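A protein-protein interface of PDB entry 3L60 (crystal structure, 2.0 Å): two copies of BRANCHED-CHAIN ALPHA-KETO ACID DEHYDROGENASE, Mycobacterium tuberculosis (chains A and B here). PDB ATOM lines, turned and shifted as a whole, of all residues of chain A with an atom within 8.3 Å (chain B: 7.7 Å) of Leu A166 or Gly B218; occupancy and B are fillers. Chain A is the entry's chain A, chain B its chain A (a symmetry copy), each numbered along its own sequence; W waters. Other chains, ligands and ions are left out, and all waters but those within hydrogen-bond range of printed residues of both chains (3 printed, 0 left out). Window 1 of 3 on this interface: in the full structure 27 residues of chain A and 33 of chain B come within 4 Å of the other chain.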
ATOM      1  N   MET A  26      -1.980  23.733  32.244  1.00  0.00           N
ATOM      2  CA  MET A  26      -2.551  22.988  31.081  1.00  0.00           C
ATOM      3  C   MET A  26      -2.877  21.527  31.495  1.00  0.00           C
ATOM      4  O   MET A  26      -4.037  21.097  31.435  1.00  0.00           O
ATOM      5  CB  MET A  26      -1.590  23.001  29.870  1.00  0.00           C
ATOM      6  CG  MET A  26      -2.068  22.182  28.612  1.00  0.00           C
ATOM      7  SD  MET A  26      -0.975  22.184  27.141  1.00  0.00           S
ATOM      8  CE  MET A  26       0.202  20.884  27.645  1.00  0.00           C
ATOM      9  N   GLY A 109      -6.814  30.536  21.867  1.00  0.00           N
ATOM     10  CA  GLY A 109      -5.452  30.070  21.978  1.00  0.00           C
ATOM     11  C   GLY A 109      -4.482  31.006  21.287  1.00  0.00           C
ATOM     12  O   GLY A 109      -4.761  31.503  20.196  1.00  0.00           O
ATOM     13  N   ALA A 110      -3.369  31.306  21.965  1.00  0.00           N
ATOM     14  CA  ALA A 110      -2.224  31.974  21.355  1.00  0.00           C
ATOM     15  C   ALA A 110      -0.950  31.179  21.725  1.00  0.00           C
ATOM     16  O   ALA A 110      -0.469  31.240  22.858  1.00  0.00           O
ATOM     17  CB  ALA A 110      -2.136  33.423  21.808  1.00  0.00           C
ATOM     18  N   ALA A 111      -0.452  30.376  20.775  1.00  0.00           N
ATOM     19  CA  ALA A 111       0.765  29.576  20.978  1.00  0.00           C
ATOM     20  C   ALA A 111       1.990  30.520  21.007  1.00  0.00           C
ATOM     21  O   ALA A 111       2.117  31.403  20.141  1.00  0.00           O
ATOM     22  CB  ALA A 111       0.913  28.485  19.867  1.00  0.00           C
ATOM     23  N   THR A 112       2.842  30.356  22.023  1.00  0.00           N
ATOM     24  CA  THR A 112       4.023  31.230  22.231  1.00  0.00           C
ATOM     25  C   THR A 112       5.249  30.391  22.605  1.00  0.00           C
ATOM     26  O   THR A 112       5.122  29.197  22.920  1.00  0.00           O
ATOM     27  CB  THR A 112       3.763  32.286  23.361  1.00  0.00           C
ATOM     28  OG1 THR A 112       3.804  31.654  24.655  1.00  0.00           O
ATOM     29  CG2 THR A 112       2.403  32.972  23.138  1.00  0.00           C
ATOM     30  N   GLY A 115       4.872  28.232  25.603  1.00  0.00           N
ATOM     31  CA  GLY A 115       3.675  27.380  25.564  1.00  0.00           C
ATOM     32  C   GLY A 115       2.449  28.121  25.037  1.00  0.00           C
ATOM     33  O   GLY A 115       2.538  29.240  24.501  1.00  0.00           O
ATOM     34  N   LEU A 116       1.290  27.499  25.176  1.00  0.00           N
ATOM     35  CA  LEU A 116       0.073  28.153  24.699  1.00  0.00           C
ATOM     36  C   LEU A 116      -0.560  28.938  25.852  1.00  0.00           C
ATOM     37  O   LEU A 116      -0.571  28.509  27.002  1.00  0.00           O
ATOM     38  CB  LEU A 116      -0.886  27.156  24.023  1.00  0.00           C
ATOM     39  CG  LEU A 116      -2.410  27.421  24.053  1.00  0.00           C
ATOM     40  CD1 LEU A 116      -3.059  27.028  22.727  1.00  0.00           C
ATOM     41  CD2 LEU A 116      -3.084  26.688  25.251  1.00  0.00           C
ATOM     42  N   SER A 161      -9.991  27.399  19.480  1.00  0.00           N
ATOM     43  CA  SER A 161      -8.672  26.859  19.210  1.00  0.00           C
ATOM     44  C   SER A 161      -8.369  26.961  17.717  1.00  0.00           C
ATOM     45  O   SER A 161      -8.996  26.275  16.880  1.00  0.00           O
ATOM     46  CB  SER A 161      -8.584  25.402  19.699  1.00  0.00           C
ATOM     47  OG  SER A 161      -7.322  24.855  19.374  1.00  0.00           O
ATOM     48  N   ASN A 162      -7.449  27.851  17.358  1.00  0.00           N
ATOM     49  CA  ASN A 162      -7.110  28.044  15.970  1.00  0.00           C
ATOM     50  C   ASN A 162      -5.902  27.165  15.571  1.00  0.00           C
ATOM     51  O   ASN A 162      -4.798  27.660  15.283  1.00  0.00           O
ATOM     52  CB  ASN A 162      -6.867  29.522  15.667  1.00  0.00           C
ATOM     53  CG  ASN A 162      -6.660  29.779  14.179  1.00  0.00           C
ATOM     54  OD1 ASN A 162      -6.906  28.910  13.328  1.00  0.00           O
ATOM     55  ND2 ASN A 162      -6.216  30.980  13.859  1.00  0.00           N
ATOM     56  N   PHE A 163      -6.126  25.853  15.536  1.00  0.00           N
ATOM     57  CA  PHE A 163      -5.056  24.946  15.127  1.00  0.00           C
ATOM     58  C   PHE A 163      -4.798  25.096  13.630  1.00  0.00           C
ATOM     59  O   PHE A 163      -3.740  24.748  13.154  1.00  0.00           O
ATOM     60  CB  PHE A 163      -5.327  23.492  15.546  1.00  0.00           C
ATOM     61  CG  PHE A 163      -6.729  23.056  15.359  1.00  0.00           C
ATOM     62  CD1 PHE A 163      -7.227  22.803  14.109  1.00  0.00           C
ATOM     63  CD2 PHE A 163      -7.566  22.866  16.455  1.00  0.00           C
ATOM     64  CE1 PHE A 163      -8.561  22.403  13.948  1.00  0.00           C
ATOM     65  CE2 PHE A 163      -8.880  22.465  16.294  1.00  0.00           C
ATOM     66  CZ  PHE A 163      -9.381  22.240  15.052  1.00  0.00           C
ATOM     67  N   GLY A 164      -5.744  25.648  12.886  1.00  0.00           N
ATOM     68  CA  GLY A 164      -5.535  25.921  11.458  1.00  0.00           C
ATOM     69  C   GLY A 164      -4.341  26.819  11.157  1.00  0.00           C
ATOM     70  O   GLY A 164      -3.639  26.621  10.167  1.00  0.00           O
ATOM     71  N   ALA A 165      -4.080  27.783  12.028  1.00  0.00           N
ATOM     72  CA  ALA A 165      -2.932  28.667  11.841  1.00  0.00           C
ATOM     73  C   ALA A 165      -1.619  27.872  11.941  1.00  0.00           C
ATOM     74  O   ALA A 165      -0.603  28.297  11.392  1.00  0.00           O
ATOM     75  CB  ALA A 165      -2.960  29.851  12.877  1.00  0.00           C
ATOM     76  N   LEU A 166      -1.674  26.693  12.597  1.00  0.00           N
ATOM     77  CA  LEU A 166      -0.510  25.825  12.758  1.00  0.00           C
ATOM     78  C   LEU A 166      -0.397  24.755  11.669  1.00  0.00           C
ATOM     79  O   LEU A 166       0.521  23.923  11.701  1.00  0.00           O
ATOM     80  CB  LEU A 166      -0.535  25.185  14.148  1.00  0.00           C
ATOM     81  CG  LEU A 166      -0.675  26.129  15.359  1.00  0.00           C
ATOM     82  CD1 LEU A 166      -0.673  25.335  16.646  1.00  0.00           C
ATOM     83  CD2 LEU A 166       0.407  27.218  15.405  1.00  0.00           C
ATOM     84  N   GLY A 167      -1.305  24.793  10.691  1.00  0.00           N
ATOM     85  CA  GLY A 167      -1.301  23.846   9.574  1.00  0.00           C
ATOM     86  C   GLY A 167      -2.164  22.599   9.727  1.00  0.00           C
ATOM     87  O   GLY A 167      -2.144  21.717   8.856  1.00  0.00           O
ATOM     88  N   VAL A 168      -2.916  22.490  10.816  1.00  0.00           N
ATOM     89  CA  VAL A 168      -3.800  21.338  11.033  1.00  0.00           C
ATOM     90  C   VAL A 168      -5.105  21.526  10.249  1.00  0.00           C
ATOM     91  O   VAL A 168      -5.800  22.559  10.402  1.00  0.00           O
ATOM     92  CB  VAL A 168      -4.092  21.133  12.540  1.00  0.00           C
ATOM     93  CG1 VAL A 168      -5.186  20.101  12.776  1.00  0.00           C
ATOM     94  CG2 VAL A 168      -2.750  20.753  13.303  1.00  0.00           C
ATOM     95  N   ASP A 169      -5.464  20.532   9.440  1.00  0.00           N
ATOM     96  CA  ASP A 169      -6.694  20.588   8.629  1.00  0.00           C
ATOM     97  C   ASP A 169      -7.964  20.467   9.445  1.00  0.00           C
ATOM     98  O   ASP A 169      -8.947  21.139   9.181  1.00  0.00           O
ATOM     99  CB  ASP A 169      -6.652  19.556   7.509  1.00  0.00           C
ATOM    100  CG  ASP A 169      -5.551  19.866   6.478  1.00  0.00           C
ATOM    101  OD1 ASP A 169      -5.542  20.983   5.905  1.00  0.00           O
ATOM    102  OD2 ASP A 169      -4.670  19.016   6.275  1.00  0.00           O
ATOM    103  N   LEU A 185     -10.939  25.757  14.712  1.00  0.00           N
ATOM    104  CA  LEU A 185     -10.839  26.308  13.358  1.00  0.00           C
ATOM    105  C   LEU A 185      -9.750  25.591  12.576  1.00  0.00           C
ATOM    106  O   LEU A 185      -8.554  25.752  12.861  1.00  0.00           O
ATOM    107  CB  LEU A 185     -10.507  27.816  13.387  1.00  0.00           C
ATOM    108  CG  LEU A 185     -11.266  28.747  14.343  1.00  0.00           C
ATOM    109  CD1 LEU A 185     -10.825  30.264  14.257  1.00  0.00           C
ATOM    110  CD2 LEU A 185     -12.748  28.638  14.038  1.00  0.00           C
ATOM    111  N   GLY A 186     -10.154  24.776  11.606  1.00  0.00           N
ATOM    112  CA  GLY A 186      -9.221  24.123  10.725  1.00  0.00           C
ATOM    113  C   GLY A 186      -8.491  25.081   9.784  1.00  0.00           C
ATOM    114  O   GLY A 186      -8.871  26.258   9.618  1.00  0.00           O
ATOM    115  N   ALA A 187      -7.422  24.580   9.174  1.00  0.00           N
ATOM    116  CA  ALA A 187      -6.652  25.390   8.228  1.00  0.00           C
ATOM    117  C   ALA A 187      -7.480  25.871   7.019  1.00  0.00           C
ATOM    118  O   ALA A 187      -8.167  25.090   6.352  1.00  0.00           O
ATOM    119  CB  ALA A 187      -5.431  24.646   7.749  1.00  0.00           C
ATOM    120  N   ILE A 188      -7.394  27.167   6.746  1.00  0.00           N
ATOM    121  CA  ILE A 188      -7.930  27.738   5.506  1.00  0.00           C
ATOM    122  C   ILE A 188      -6.950  27.509   4.384  1.00  0.00           C
ATOM    123  O   ILE A 188      -5.807  27.949   4.460  1.00  0.00           O
ATOM    124  CB  ILE A 188      -8.191  29.241   5.630  1.00  0.00           C
ATOM    125  CG1 ILE A 188      -9.279  29.505   6.690  1.00  0.00           C
ATOM    126  CG2 ILE A 188      -8.655  29.812   4.272  1.00  0.00           C
ATOM    127  CD1 ILE A 188      -9.421  30.994   7.077  1.00  0.00           C
ATOM    128  N   ALA B  40      -6.686  14.710  22.912  1.00  0.00           N
ATOM    129  CA  ALA B  40      -7.131  15.598  21.840  1.00  0.00           C
ATOM    130  C   ALA B  40      -6.672  14.970  20.517  1.00  0.00           C
ATOM    131  O   ALA B  40      -5.859  14.024  20.495  1.00  0.00           O
ATOM    132  CB  ALA B  40      -6.555  17.011  22.044  1.00  0.00           C
ATOM    133  N   ALA B  42      -5.572  15.728  16.226  1.00  0.00           N
ATOM    134  CA  ALA B  42      -5.166  16.619  15.112  1.00  0.00           C
ATOM    135  C   ALA B  42      -5.007  15.761  13.863  1.00  0.00           C
ATOM    136  O   ALA B  42      -4.371  14.689  13.907  1.00  0.00           O
ATOM    137  CB  ALA B  42      -3.866  17.339  15.431  1.00  0.00           C
ATOM    138  N   VAL B  44      -4.247  15.819   9.452  1.00  0.00           N
ATOM    139  CA  VAL B  44      -3.735  16.465   8.241  1.00  0.00           C
ATOM    140  C   VAL B  44      -3.935  15.576   7.051  1.00  0.00           C
ATOM    141  O   VAL B  44      -3.730  14.349   7.116  1.00  0.00           O
ATOM    142  CB  VAL B  44      -2.183  16.847   8.303  1.00  0.00           C
ATOM    143  CG1 VAL B  44      -1.931  17.993   9.287  1.00  0.00           C
ATOM    144  CG2 VAL B  44      -1.294  15.625   8.558  1.00  0.00           C
ATOM    145  N   PHE B 211      -3.491  12.416  20.997  1.00  0.00           N
ATOM    146  CA  PHE B 211      -2.449  12.647  21.951  1.00  0.00           C
ATOM    147  C   PHE B 211      -2.952  13.006  23.344  1.00  0.00           C
ATOM    148  O   PHE B 211      -4.008  13.613  23.523  1.00  0.00           O
ATOM    149  CB  PHE B 211      -1.509  13.747  21.429  1.00  0.00           C
ATOM    150  CG  PHE B 211      -2.178  15.088  21.144  1.00  0.00           C
ATOM    151  CD1 PHE B 211      -2.026  16.145  22.026  1.00  0.00           C
ATOM    152  CD2 PHE B 211      -2.873  15.307  19.961  1.00  0.00           C
ATOM    153  CE1 PHE B 211      -2.588  17.370  21.774  1.00  0.00           C
ATOM    154  CE2 PHE B 211      -3.460  16.536  19.705  1.00  0.00           C
ATOM    155  CZ  PHE B 211      -3.312  17.569  20.612  1.00  0.00           C
ATOM    156  N   HIS B 213      -3.026  15.257  26.112  1.00  0.00           N
ATOM    157  CA  HIS B 213      -2.880  16.724  26.109  1.00  0.00           C
ATOM    158  C   HIS B 213      -2.240  17.236  27.431  1.00  0.00           C
ATOM    159  O   HIS B 213      -1.987  18.415  27.569  1.00  0.00           O
ATOM    160  CB  HIS B 213      -4.227  17.420  25.819  1.00  0.00           C
ATOM    161  CG  HIS B 213      -4.089  18.775  25.175  1.00  0.00           C
ATOM    162  ND1 HIS B 213      -3.125  19.693  25.543  1.00  0.00           N
ATOM    163  CD2 HIS B 213      -4.842  19.391  24.233  1.00  0.00           C
ATOM    164  CE1 HIS B 213      -3.272  20.798  24.837  1.00  0.00           C
ATOM    165  NE2 HIS B 213      -4.310  20.644  24.040  1.00  0.00           N
ATOM    166  N   VAL B 216       1.594  16.680  25.499  1.00  0.00           N
ATOM    167  CA  VAL B 216       1.841  17.322  24.226  1.00  0.00           C
ATOM    168  C   VAL B 216       0.841  18.460  24.080  1.00  0.00           C
ATOM    169  O   VAL B 216      -0.357  18.290  24.396  1.00  0.00           O
ATOM    170  CB  VAL B 216       1.669  16.340  23.060  1.00  0.00           C
ATOM    171  CG1 VAL B 216       2.074  17.006  21.712  1.00  0.00           C
ATOM    172  CG2 VAL B 216       2.495  15.053  23.307  1.00  0.00           C
ATOM    173  N   ASP B 217       1.316  19.616  23.622  1.00  0.00           N
ATOM    174  CA  ASP B 217       0.416  20.742  23.339  1.00  0.00           C
ATOM    175  C   ASP B 217       0.117  20.845  21.847  1.00  0.00           C
ATOM    176  O   ASP B 217       0.648  20.084  21.037  1.00  0.00           O
ATOM    177  CB  ASP B 217       0.888  22.083  23.973  1.00  0.00           C
ATOM    178  CG  ASP B 217       2.102  22.709  23.298  1.00  0.00           C
ATOM    179  OD1 ASP B 217       2.339  22.491  22.102  1.00  0.00           O
ATOM    180  OD2 ASP B 217       2.809  23.494  23.989  1.00  0.00           O
ATOM    181  N   GLY B 218      -0.788  21.747  21.488  1.00  0.00           N
ATOM    182  CA  GLY B 218      -1.249  21.818  20.098  1.00  0.00           C
ATOM    183  C   GLY B 218      -0.164  22.248  19.157  1.00  0.00           C
ATOM    184  O   GLY B 218      -0.098  21.741  18.044  1.00  0.00           O
ATOM    185  N   ALA B 219       0.702  23.173  19.589  1.00  0.00           N
ATOM    186  CA  ALA B 219       1.790  23.630  18.748  1.00  0.00           C
ATOM    187  C   ALA B 219       2.745  22.484  18.474  1.00  0.00           C
ATOM    188  O   ALA B 219       3.187  22.287  17.349  1.00  0.00           O
ATOM    189  CB  ALA B 219       2.529  24.826  19.395  1.00  0.00           C
ATOM    190  N   GLN B 220       3.022  21.683  19.496  1.00  0.00           N
ATOM    191  CA  GLN B 220       3.911  20.519  19.328  1.00  0.00           C
ATOM    192  C   GLN B 220       3.356  19.429  18.394  1.00  0.00           C
ATOM    193  O   GLN B 220       4.051  18.929  17.481  1.00  0.00           O
ATOM    194  CB  GLN B 220       4.236  19.963  20.710  1.00  0.00           C
ATOM    195  CG  GLN B 220       5.126  20.918  21.564  1.00  0.00           C
ATOM    196  CD  GLN B 220       5.217  20.477  23.028  1.00  0.00           C
ATOM    197  OE1 GLN B 220       4.271  19.931  23.586  1.00  0.00           O
ATOM    198  NE2 GLN B 220       6.377  20.706  23.646  1.00  0.00           N
ATOM    199  N   VAL B 221       2.087  19.056  18.590  1.00  0.00           N
ATOM    200  CA  VAL B 221       1.458  18.126  17.650  1.00  0.00           C
ATOM    201  C   VAL B 221       1.399  18.678  16.213  1.00  0.00           C
ATOM    202  O   VAL B 221       1.640  17.946  15.270  1.00  0.00           O
ATOM    203  CB  VAL B 221       0.042  17.597  18.128  1.00  0.00           C
ATOM    204  CG1 VAL B 221      -1.007  18.662  18.007  1.00  0.00           C
ATOM    205  CG2 VAL B 221      -0.349  16.345  17.336  1.00  0.00           C
ATOM    206  N   ALA B 222       1.109  19.972  16.039  1.00  0.00           N
ATOM    207  CA  ALA B 222       1.029  20.541  14.686  1.00  0.00           C
ATOM    208  C   ALA B 222       2.392  20.480  14.017  1.00  0.00           C
ATOM    209  O   ALA B 222       2.517  20.162  12.809  1.00  0.00           O
ATOM    210  CB  ALA B 222       0.510  22.015  14.716  1.00  0.00           C
ATOM    211  N   GLN B 223       3.425  20.806  14.783  1.00  0.00           N
ATOM    212  CA  GLN B 223       4.785  20.793  14.209  1.00  0.00           C
ATOM    213  C   GLN B 223       5.145  19.378  13.747  1.00  0.00           C
ATOM    214  O   GLN B 223       5.692  19.174  12.666  1.00  0.00           O
ATOM    215  CB  GLN B 223       5.833  21.321  15.193  1.00  0.00           C
ATOM    216  CG  GLN B 223       7.297  21.144  14.696  1.00  0.00           C
ATOM    217  CD  GLN B 223       8.297  21.712  15.670  1.00  0.00           C
ATOM    218  OE1 GLN B 223       8.204  22.872  16.040  1.00  0.00           O
ATOM    219  NE2 GLN B 223       9.221  20.872  16.145  1.00  0.00           N
ATOM    220  N   PHE B 224       4.816  18.396  14.576  1.00  0.00           N
ATOM    221  CA  PHE B 224       5.073  16.989  14.273  1.00  0.00           C
ATOM    222  C   PHE B 224       4.311  16.566  13.017  1.00  0.00           C
ATOM    223  O   PHE B 224       4.855  15.981  12.060  1.00  0.00           O
ATOM    224  CB  PHE B 224       4.651  16.153  15.499  1.00  0.00           C
ATOM    225  CG  PHE B 224       4.507  14.681  15.240  1.00  0.00           C
ATOM    226  CD1 PHE B 224       5.601  13.912  14.874  1.00  0.00           C
ATOM    227  CD2 PHE B 224       3.279  14.051  15.408  1.00  0.00           C
ATOM    228  CE1 PHE B 224       5.490  12.548  14.662  1.00  0.00           C
ATOM    229  CE2 PHE B 224       3.148  12.664  15.197  1.00  0.00           C
ATOM    230  CZ  PHE B 224       4.247  11.920  14.822  1.00  0.00           C
ATOM    231  N   MET B 225       3.034  16.921  12.970  1.00  0.00           N
ATOM    232  CA  MET B 225       2.208  16.427  11.876  1.00  0.00           C
ATOM    233  C   MET B 225       2.562  17.120  10.558  1.00  0.00           C
ATOM    234  O   MET B 225       2.578  16.485   9.519  1.00  0.00           O
ATOM    235  CB  MET B 225       0.705  16.567  12.210  1.00  0.00           C
ATOM    236  CG  MET B 225       0.292  15.568  13.380  1.00  0.00           C
ATOM    237  SD  MET B 225       0.281  13.841  12.818  1.00  0.00           S
ATOM    238  CE  MET B 225      -1.382  13.804  12.096  1.00  0.00           C
ATOM    239  N   CYS B 226       2.790  18.421  10.612  1.00  0.00           N
ATOM    240  CA  CYS B 226       3.246  19.130   9.424  1.00  0.00           C
ATOM    241  C   CYS B 226       4.577  18.568   8.879  1.00  0.00           C
ATOM    242  O   CYS B 226       4.748  18.458   7.659  1.00  0.00           O
ATOM    243  CB  CYS B 226       3.361  20.614   9.713  1.00  0.00           C
ATOM    244  SG  CYS B 226       1.731  21.398   9.874  1.00  0.00           S
ATOM    245  N   ARG B 229       3.768  15.222   7.287  1.00  0.00           N
ATOM    246  CA  ARG B 229       3.160  15.465   5.970  1.00  0.00           C
ATOM    247  C   ARG B 229       4.212  15.840   4.899  1.00  0.00           C
ATOM    248  O   ARG B 229       4.198  15.331   3.766  1.00  0.00           O
ATOM    249  CB  ARG B 229       2.191  16.631   6.082  1.00  0.00           C
ATOM    250  CG  ARG B 229       1.586  17.015   4.738  1.00  0.00           C
ATOM    251  CD  ARG B 229       0.711  18.210   4.895  1.00  0.00           C
ATOM    252  NE  ARG B 229       1.523  19.326   5.338  1.00  0.00           N
ATOM    253  CZ  ARG B 229       1.102  20.340   6.080  1.00  0.00           C
ATOM    254  NH1 ARG B 229      -0.160  20.429   6.510  1.00  0.00           N
ATOM    255  NH2 ARG B 229       1.977  21.284   6.389  1.00  0.00           N
HETATM  256  O   HOH W   1      -3.153  22.195   6.299  1.00  0.00           O
HETATM  257  O   HOH W   2       1.303  24.963  26.256  1.00  0.00           O
HETATM  258  O   HOH W   3      -2.428  19.094   5.107  1.00  0.00           O
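N of Ala A187 lies within hydrogen-bond range of O of Val A168 (2.9 Å). A ring nitrogen (ND1) of His B213 is in hydrogen-bond range of the backbone carbonyl oxygen (O) of Val B216, at 3.3 Å. The side-chain carboxylate (OD1) of Asp B217 sits at hydrogen-bond distance from the backbone NH (N) of Ala B219 (3.1 Å). The backbone NH (N) of Gln B220 is in hydrogen-bond range of the side-chain carboxylate (OD1) of Asp B217, at 2.8 Å. O of Ala B222 lies close to SG of Cys B226 (3.3 Å). The guanidinium group (NH2) of Arg B229 sits at hydrogen-bond distance from the side-chain sulfur (SG) of Cys B226, at 3.5 Å.
Of the 17 printed residues of chain B, 8 touch a printed residue of chain A. Printed residues of chain B that touch a printed residue of chain A: Val B44, His B213, Asp B217, Gly B218, Ala B219, Ala B222, Cys B226 and Arg B229. Hydrophobic or aromatic side chains of chain B within 4 Å of the printed part of chain A: Val B44, His B213 and Ala B222. Among the printed residues, 11 pairs touch across the chains.
Water W3 lies within hydrogen-bond range of the side-chain carboxylate of Asp A169 (2.5 Å) and the guanidinium group of Arg B229 (3.0 Å). Water W1 lies within hydrogen-bond range of OD1 of Asp A169, O of Gly A167 and NH1 of Arg B229. Water W2 lies within hydrogen-bond range of the backbone NH (N) of Leu A116 (2.8 Å), the side-chain carboxylate (OD2) of Asp B217 (3.1 Å) and the side-chain sulfur (SD) of Met A26 (3.7 Å).
Of the printed residues of chain B, Met A26 touches His B213 (3.3 Å) and Asp B217 (3.7 Å). Leu A166 touches four residues of chain B. Gly B218 touches just one residue of chain A: Leu A166 (3.9 Å). Ala B219 touches one residue of chain A. Printed residues of chain A within 4 Å of Arg B229: Gly A167. The nearest residue of chain B that does not touch Leu A166 is Gln B223 (5.3 Å). The nearest residue of chain A that does not touch Gly B218 is Val A168 (5.5 Å).
The side-chain sulfur (SD) of Met A26 sits close to a ring nitrogen (ND1) of His B213, at 3.7 Å. The backbone carbonyl oxygen of Leu A166 lies within hydrogen-bond range of the side-chain sulfur of Cys B226 (3.3 Å). The guanidinium group (NH1) of Arg B229 is in hydrogen-bond range of the backbone carbonyl oxygen (O) of Gly A167.
Among the printed residues, merely in contact across the chains: Asp A169 with Val B44 (3.4 Å), Leu A166 with Ala B222 (3.4 Å), Leu A166 with Ala B219 (3.7 Å), Met A26 with Asp B217 (3.7 Å), Gly A167 with Val B44 (3.8 Å), Val A168 with Ala B222 (3.8 Å), Leu A166 with Gly B218 (3.9 Å) and Gly A167 with Cys B226 (3.9 Å).
No position is printed for both chains. Of the 11 pairs that touch across the chains among the printed residues, none has its exchanged pair printed and touching as well.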
